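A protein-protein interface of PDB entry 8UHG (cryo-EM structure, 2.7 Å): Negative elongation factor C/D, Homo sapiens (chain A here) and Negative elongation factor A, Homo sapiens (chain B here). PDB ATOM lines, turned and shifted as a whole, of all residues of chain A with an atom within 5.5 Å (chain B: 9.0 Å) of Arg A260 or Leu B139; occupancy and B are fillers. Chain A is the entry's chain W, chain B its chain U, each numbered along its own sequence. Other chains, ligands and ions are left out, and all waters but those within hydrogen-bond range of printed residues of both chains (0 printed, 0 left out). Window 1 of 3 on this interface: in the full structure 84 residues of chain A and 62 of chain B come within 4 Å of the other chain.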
ATOM      1  N   GLY A 255      12.976  -7.300  26.753  1.00  0.00           N
ATOM      2  CA  GLY A 255      12.080  -7.220  25.611  1.00  0.00           C
ATOM      3  C   GLY A 255      11.416  -8.537  25.258  1.00  0.00           C
ATOM      4  O   GLY A 255      10.438  -8.546  24.504  1.00  0.00           O
ATOM      5  N   SER A 256      11.938  -9.653  25.775  1.00  0.00           N
ATOM      6  CA  SER A 256      11.238 -10.928  25.674  1.00  0.00           C
ATOM      7  C   SER A 256       9.833 -10.829  26.264  1.00  0.00           C
ATOM      8  O   SER A 256       8.876 -11.387  25.713  1.00  0.00           O
ATOM      9  CB  SER A 256      12.051 -12.018  26.383  1.00  0.00           C
ATOM     10  OG  SER A 256      11.613 -12.191  27.718  1.00  0.00           O
ATOM     11  N   ALA A 257       9.683 -10.094  27.369  1.00  0.00           N
ATOM     12  CA  ALA A 257       8.364  -9.922  27.974  1.00  0.00           C
ATOM     13  C   ALA A 257       7.461  -9.045  27.115  1.00  0.00           C
ATOM     14  O   ALA A 257       6.248  -9.273  27.048  1.00  0.00           O
ATOM     15  CB  ALA A 257       8.504  -9.332  29.377  1.00  0.00           C
ATOM     16  N   VAL A 258       8.025  -8.032  26.455  1.00  0.00           N
ATOM     17  CA  VAL A 258       7.217  -7.213  25.557  1.00  0.00           C
ATOM     18  C   VAL A 258       6.773  -8.036  24.354  1.00  0.00           C
ATOM     19  O   VAL A 258       5.655  -7.880  23.854  1.00  0.00           O
ATOM     20  CB  VAL A 258       7.990  -5.951  25.129  1.00  0.00           C
ATOM     21  CG1 VAL A 258       7.141  -5.120  24.169  1.00  0.00           C
ATOM     22  CG2 VAL A 258       8.398  -5.124  26.351  1.00  0.00           C
ATOM     23  N   ARG A 259       7.645  -8.926  23.873  1.00  0.00           N
ATOM     24  CA  ARG A 259       7.272  -9.857  22.811  1.00  0.00           C
ATOM     25  C   ARG A 259       6.146 -10.781  23.266  1.00  0.00           C
ATOM     26  O   ARG A 259       5.206 -11.054  22.507  1.00  0.00           O
ATOM     27  CB  ARG A 259       8.511 -10.656  22.404  1.00  0.00           C
ATOM     28  CG  ARG A 259       8.346 -11.656  21.272  1.00  0.00           C
ATOM     29  CD  ARG A 259       9.696 -12.306  20.993  1.00  0.00           C
ATOM     30  NE  ARG A 259       9.608 -13.489  20.142  1.00  0.00           N
ATOM     31  CZ  ARG A 259      10.573 -14.388  19.985  1.00  0.00           C
ATOM     32  NH1 ARG A 259      11.730 -14.296  20.627  1.00  0.00           N
ATOM     33  NH2 ARG A 259      10.374 -15.413  19.162  1.00  0.00           N
ATOM     34  N   ARG A 260       6.236 -11.272  24.505  1.00  0.00           N
ATOM     35  CA  ARG A 260       5.167 -12.080  25.092  1.00  0.00           C
ATOM     36  C   ARG A 260       3.848 -11.315  25.103  1.00  0.00           C
ATOM     37  O   ARG A 260       2.806 -11.839  24.691  1.00  0.00           O
ATOM     38  CB  ARG A 260       5.578 -12.502  26.510  1.00  0.00           C
ATOM     39  CG  ARG A 260       4.468 -12.929  27.483  1.00  0.00           C
ATOM     40  CD  ARG A 260       3.615 -14.070  26.964  1.00  0.00           C
ATOM     41  NE  ARG A 260       2.808 -14.662  28.027  1.00  0.00           N
ATOM     42  CZ  ARG A 260       3.226 -15.579  28.894  1.00  0.00           C
ATOM     43  NH1 ARG A 260       4.461 -16.062  28.865  1.00  0.00           N
ATOM     44  NH2 ARG A 260       2.384 -16.019  29.823  1.00  0.00           N
ATOM     45  N   ILE A 261       3.879 -10.065  25.564  1.00  0.00           N
ATOM     46  CA  ILE A 261       2.648  -9.286  25.660  1.00  0.00           C
ATOM     47  C   ILE A 261       2.104  -8.970  24.270  1.00  0.00           C
ATOM     48  O   ILE A 261       0.885  -8.915  24.073  1.00  0.00           O
ATOM     49  CB  ILE A 261       2.877  -8.005  26.484  1.00  0.00           C
ATOM     50  CG1 ILE A 261       3.209  -8.346  27.944  1.00  0.00           C
ATOM     51  CG2 ILE A 261       1.634  -7.110  26.442  1.00  0.00           C
ATOM     52  CD1 ILE A 261       3.970  -7.260  28.659  1.00  0.00           C
ATOM     53  N   ALA A 262       2.985  -8.749  23.290  1.00  0.00           N
ATOM     54  CA  ALA A 262       2.531  -8.540  21.917  1.00  0.00           C
ATOM     55  C   ALA A 262       1.839  -9.782  21.374  1.00  0.00           C
ATOM     56  O   ALA A 262       0.803  -9.685  20.705  1.00  0.00           O
ATOM     57  CB  ALA A 262       3.711  -8.158  21.025  1.00  0.00           C
ATOM     58  N   GLN A 263       2.403 -10.962  21.644  1.00  0.00           N
ATOM     59  CA  GLN A 263       1.756 -12.203  21.228  1.00  0.00           C
ATOM     60  C   GLN A 263       0.408 -12.376  21.919  1.00  0.00           C
ATOM     61  O   GLN A 263      -0.551 -12.865  21.313  1.00  0.00           O
ATOM     62  CB  GLN A 263       2.673 -13.390  21.520  1.00  0.00           C
ATOM     63  CG  GLN A 263       3.913 -13.442  20.631  1.00  0.00           C
ATOM     64  CD  GLN A 263       4.998 -14.352  21.180  1.00  0.00           C
ATOM     65  OE1 GLN A 263       5.220 -14.418  22.389  1.00  0.00           O
ATOM     66  NE2 GLN A 263       5.683 -15.057  20.287  1.00  0.00           N
ATOM     67  N   GLU A 264       0.318 -11.979  23.190  1.00  0.00           N
ATOM     68  CA  GLU A 264      -0.956 -12.045  23.903  1.00  0.00           C
ATOM     69  C   GLU A 264      -1.985 -11.099  23.287  1.00  0.00           C
ATOM     70  O   GLU A 264      -3.167 -11.445  23.166  1.00  0.00           O
ATOM     71  CB  GLU A 264      -0.746 -11.709  25.379  1.00  0.00           C
ATOM     72  CG  GLU A 264       0.129 -12.697  26.147  1.00  0.00           C
ATOM     73  CD  GLU A 264      -0.648 -13.867  26.715  1.00  0.00           C
ATOM     74  OE1 GLU A 264      -1.733 -14.184  26.185  1.00  0.00           O
ATOM     75  OE2 GLU A 264      -0.170 -14.472  27.698  1.00  0.00           O
ATOM     76  N   VAL A 265      -1.557  -9.895  22.907  1.00  0.00           N
ATOM     77  CA  VAL A 265      -2.478  -8.951  22.281  1.00  0.00           C
ATOM     78  C   VAL A 265      -2.913  -9.475  20.920  1.00  0.00           C
ATOM     79  O   VAL A 265      -4.055  -9.266  20.503  1.00  0.00           O
ATOM     80  CB  VAL A 265      -1.844  -7.548  22.164  1.00  0.00           C
ATOM     81  CG1 VAL A 265      -2.792  -6.584  21.437  1.00  0.00           C
ATOM     82  CG2 VAL A 265      -1.471  -6.972  23.539  1.00  0.00           C
ATOM     83  N   PRO A 331       3.030 -19.348  19.094  1.00  0.00           N
ATOM     84  CA  PRO A 331       2.226 -20.179  20.017  1.00  0.00           C
ATOM     85  C   PRO A 331       0.930 -20.709  19.422  1.00  0.00           C
ATOM     86  O   PRO A 331       0.621 -21.900  19.578  1.00  0.00           O
ATOM     87  CB  PRO A 331       1.956 -19.230  21.195  1.00  0.00           C
ATOM     88  CG  PRO A 331       2.841 -18.061  20.988  1.00  0.00           C
ATOM     89  CD  PRO A 331       3.016 -17.939  19.530  1.00  0.00           C
ATOM     90  N   SER B 134      13.141 -11.798  36.122  1.00  0.00           N
ATOM     91  CA  SER B 134      11.910 -12.579  35.980  1.00  0.00           C
ATOM     92  C   SER B 134      11.072 -12.101  34.795  1.00  0.00           C
ATOM     93  O   SER B 134       9.839 -12.132  34.839  1.00  0.00           O
ATOM     94  CB  SER B 134      11.079 -12.556  37.268  1.00  0.00           C
ATOM     95  OG  SER B 134       9.785 -13.092  37.051  1.00  0.00           O
ATOM     96  N   ALA B 135      11.735 -11.656  33.727  1.00  0.00           N
ATOM     97  CA  ALA B 135      11.036 -11.248  32.515  1.00  0.00           C
ATOM     98  C   ALA B 135      10.413 -12.480  31.877  1.00  0.00           C
ATOM     99  O   ALA B 135      11.126 -13.343  31.353  1.00  0.00           O
ATOM    100  CB  ALA B 135      11.994 -10.551  31.552  1.00  0.00           C
ATOM    101  N   MET B 136       9.085 -12.574  31.953  1.00  0.00           N
ATOM    102  CA  MET B 136       8.338 -13.696  31.396  1.00  0.00           C
ATOM    103  C   MET B 136       8.630 -13.872  29.912  1.00  0.00           C
ATOM    104  O   MET B 136       8.322 -12.995  29.100  1.00  0.00           O
ATOM    105  CB  MET B 136       6.834 -13.506  31.629  1.00  0.00           C
ATOM    106  CG  MET B 136       6.223 -12.194  31.108  1.00  0.00           C
ATOM    107  SD  MET B 136       4.603 -11.861  31.837  1.00  0.00           S
ATOM    108  CE  MET B 136       3.631 -13.204  31.162  1.00  0.00           C
ATOM    109  N   LEU B 137       9.223 -15.005  29.553  1.00  0.00           N
ATOM    110  CA  LEU B 137       9.652 -15.228  28.188  1.00  0.00           C
ATOM    111  C   LEU B 137       8.444 -15.364  27.262  1.00  0.00           C
ATOM    112  O   LEU B 137       7.314 -15.534  27.728  1.00  0.00           O
ATOM    113  CB  LEU B 137      10.513 -16.486  28.093  1.00  0.00           C
ATOM    114  CG  LEU B 137      11.972 -16.428  28.554  1.00  0.00           C
ATOM    115  CD1 LEU B 137      12.572 -17.829  28.527  1.00  0.00           C
ATOM    116  CD2 LEU B 137      12.791 -15.487  27.682  1.00  0.00           C
ATOM    117  N   PRO B 138       8.651 -15.256  25.945  1.00  0.00           N
ATOM    118  CA  PRO B 138       7.590 -15.620  25.002  1.00  0.00           C
ATOM    119  C   PRO B 138       7.116 -17.048  25.208  1.00  0.00           C
ATOM    120  O   PRO B 138       7.796 -17.884  25.805  1.00  0.00           O
ATOM    121  CB  PRO B 138       8.258 -15.447  23.635  1.00  0.00           C
ATOM    122  CG  PRO B 138       9.268 -14.399  23.852  1.00  0.00           C
ATOM    123  CD  PRO B 138       9.762 -14.571  25.260  1.00  0.00           C
ATOM    124  N   LEU B 139       5.930 -17.324  24.683  1.00  0.00           N
ATOM    125  CA  LEU B 139       5.281 -18.609  24.885  1.00  0.00           C
ATOM    126  C   LEU B 139       5.840 -19.701  23.978  1.00  0.00           C
ATOM    127  O   LEU B 139       5.409 -20.853  24.091  1.00  0.00           O
ATOM    128  CB  LEU B 139       3.770 -18.467  24.666  1.00  0.00           C
ATOM    129  CG  LEU B 139       3.087 -17.260  25.341  1.00  0.00           C
ATOM    130  CD1 LEU B 139       2.895 -16.055  24.393  1.00  0.00           C
ATOM    131  CD2 LEU B 139       1.751 -17.666  25.960  1.00  0.00           C
ATOM    132  N   GLU B 140       6.783 -19.374  23.088  1.00  0.00           N
ATOM    133  CA  GLU B 140       7.406 -20.402  22.259  1.00  0.00           C
ATOM    134  C   GLU B 140       8.345 -21.292  23.062  1.00  0.00           C
ATOM    135  O   GLU B 140       8.459 -22.486  22.767  1.00  0.00           O
ATOM    136  CB  GLU B 140       8.177 -19.772  21.095  1.00  0.00           C
ATOM    137  CG  GLU B 140       9.219 -18.713  21.473  1.00  0.00           C
ATOM    138  CD  GLU B 140      10.115 -18.328  20.313  1.00  0.00           C
ATOM    139  OE1 GLU B 140       9.700 -18.502  19.150  1.00  0.00           O
ATOM    140  OE2 GLU B 140      11.239 -17.847  20.568  1.00  0.00           O
ATOM    141  N   CYS B 141       9.017 -20.733  24.073  1.00  0.00           N
ATOM    142  CA  CYS B 141      10.076 -21.442  24.788  1.00  0.00           C
ATOM    143  C   CYS B 141       9.581 -22.697  25.498  1.00  0.00           C
ATOM    144  O   CYS B 141      10.390 -23.583  25.796  1.00  0.00           O
ATOM    145  CB  CYS B 141      10.717 -20.505  25.810  1.00  0.00           C
ATOM    146  SG  CYS B 141       9.689 -20.228  27.266  1.00  0.00           S
ATOM    147  N   GLN B 142       8.280 -22.787  25.783  1.00  0.00           N
ATOM    148  CA  GLN B 142       7.746 -23.934  26.509  1.00  0.00           C
ATOM    149  C   GLN B 142       7.928 -25.227  25.723  1.00  0.00           C
ATOM    150  O   GLN B 142       8.181 -26.287  26.309  1.00  0.00           O
ATOM    151  CB  GLN B 142       6.263 -23.710  26.812  1.00  0.00           C
ATOM    152  CG  GLN B 142       5.935 -22.463  27.623  1.00  0.00           C
ATOM    153  CD  GLN B 142       4.449 -22.175  27.660  1.00  0.00           C
ATOM    154  OE1 GLN B 142       3.638 -22.969  27.184  1.00  0.00           O
ATOM    155  NE2 GLN B 142       4.083 -21.030  28.225  1.00  0.00           N
ATOM    156  N   TYR B 143       7.813 -25.159  24.398  1.00  0.00           N
ATOM    157  CA  TYR B 143       7.684 -26.346  23.560  1.00  0.00           C
ATOM    158  C   TYR B 143       9.024 -26.827  23.009  1.00  0.00           C
ATOM    159  O   TYR B 143       9.050 -27.807  22.258  1.00  0.00           O
ATOM    160  CB  TYR B 143       6.728 -26.086  22.374  1.00  0.00           C
ATOM    161  CG  TYR B 143       5.250 -25.749  22.661  1.00  0.00           C
ATOM    162  CD1 TYR B 143       4.797 -25.334  23.911  1.00  0.00           C
ATOM    163  CD2 TYR B 143       4.307 -25.844  21.647  1.00  0.00           C
ATOM    164  CE1 TYR B 143       3.473 -25.027  24.133  1.00  0.00           C
ATOM    165  CE2 TYR B 143       2.975 -25.542  21.874  1.00  0.00           C
ATOM    166  CZ  TYR B 143       2.566 -25.136  23.114  1.00  0.00           C
ATOM    167  OH  TYR B 143       1.244 -24.834  23.333  1.00  0.00           O
ATOM    168  N   LEU B 144      10.129 -26.180  23.375  1.00  0.00           N
ATOM    169  CA  LEU B 144      11.434 -26.405  22.771  1.00  0.00           C
ATOM    170  C   LEU B 144      12.301 -27.244  23.700  1.00  0.00           C
ATOM    171  O   LEU B 144      12.167 -27.183  24.925  1.00  0.00           O
ATOM    172  CB  LEU B 144      12.135 -25.074  22.482  1.00  0.00           C
ATOM    173  CG  LEU B 144      11.245 -23.897  22.068  1.00  0.00           C
ATOM    174  CD1 LEU B 144      12.082 -22.652  21.812  1.00  0.00           C
ATOM    175  CD2 LEU B 144      10.398 -24.265  20.850  1.00  0.00           C
ATOM    176  N   ALA B 153      16.427 -18.679  23.555  1.00  0.00           N
ATOM    177  CA  ALA B 153      15.408 -18.180  24.472  1.00  0.00           C
ATOM    178  C   ALA B 153      15.934 -17.890  25.874  1.00  0.00           C
ATOM    179  O   ALA B 153      15.135 -17.541  26.750  1.00  0.00           O
ATOM    180  CB  ALA B 153      14.253 -19.180  24.556  1.00  0.00           C
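Of the printed residues of chain B, Ala A257 touches Met B136 (3.3 Å). Printed residues of chain B within 4 Å of Arg A260: Met B136 (3.3 Å), Leu B137 (3.1 Å) and Leu B139 (3.3 Å). Printed residues of chain B within 4 Å of Gln A263: Pro B138 (3.4 Å) and Leu B139 (3.5 Å). Of the printed residues of chain B, Pro A331 touches Leu B139. Printed residues of chain A within 4 Å of Ala B135: Ser A256 (3.8 Å). Printed residues of chain A within 4 Å of Met B136: Ser A256, Ala A257 and Arg A260. Of chain A, only Arg A260, Gln A263 and Pro A331 come within 4 Å of Leu B139. Tyr B143 touches none of the printed residues of chain A. The nearest printed residue of chain B that does not touch Arg A260 is Pro B138 (4.01 Å). The nearest printed residue of chain A that does not touch Glu B140 is Pro A331 (4.7 Å).
The guanidinium group (NH1) of Arg A260 is in hydrogen-bond range of the backbone carbonyl oxygen (O) of Leu B137, 3.1 Å away. NH2 of Arg A259 lies within salt-bridge range of OE2 of Glu B140.
The side-chain sulfur (SG) of Cys B141 lies within hydrogen-bond range of the backbone carbonyl oxygen (O) of Pro B138 (3.3 Å). O of Arg A259 sits close to OE1 of Gln A263. OE2 of Glu A264 is in salt-bridge range of NE of Arg A260.
Of the 12 printed residues of chain A, 6 touch a printed residue of chain B. Among the printed residues, 13 pairs touch across the chains. Among the printed residues, Asp or Glu carboxylates within 4 Å of a Lys or Arg side-chain nitrogen of the other chain: Arg A259 with Glu B140 (2.9 Å).
Ala B135 touches Ser A256. OG of Ser A256 touches O of Met B136, 3.7 Å away. OG of Ser A256 touches CD2 of Leu B137, 3.5 Å away. Pro B138 touches Ser A256 (CD to O, 3.3 Å). O of Met B136 touches CA of Ala A257, 3.3 Å away. CG of Pro B138 touches CD of Arg A259, at 3.6 Å. Arg A260 touches Met B136 (CZ to CE, 3.3 Å). OE1 of Gln A263 touches CB of Pro B138, at 3.4 Å. Leu B139 touches Gln A263 (CD1 to OE1, 3.5 Å). CG of Pro A331 touches CB of Leu B139, 3.8 Å away.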
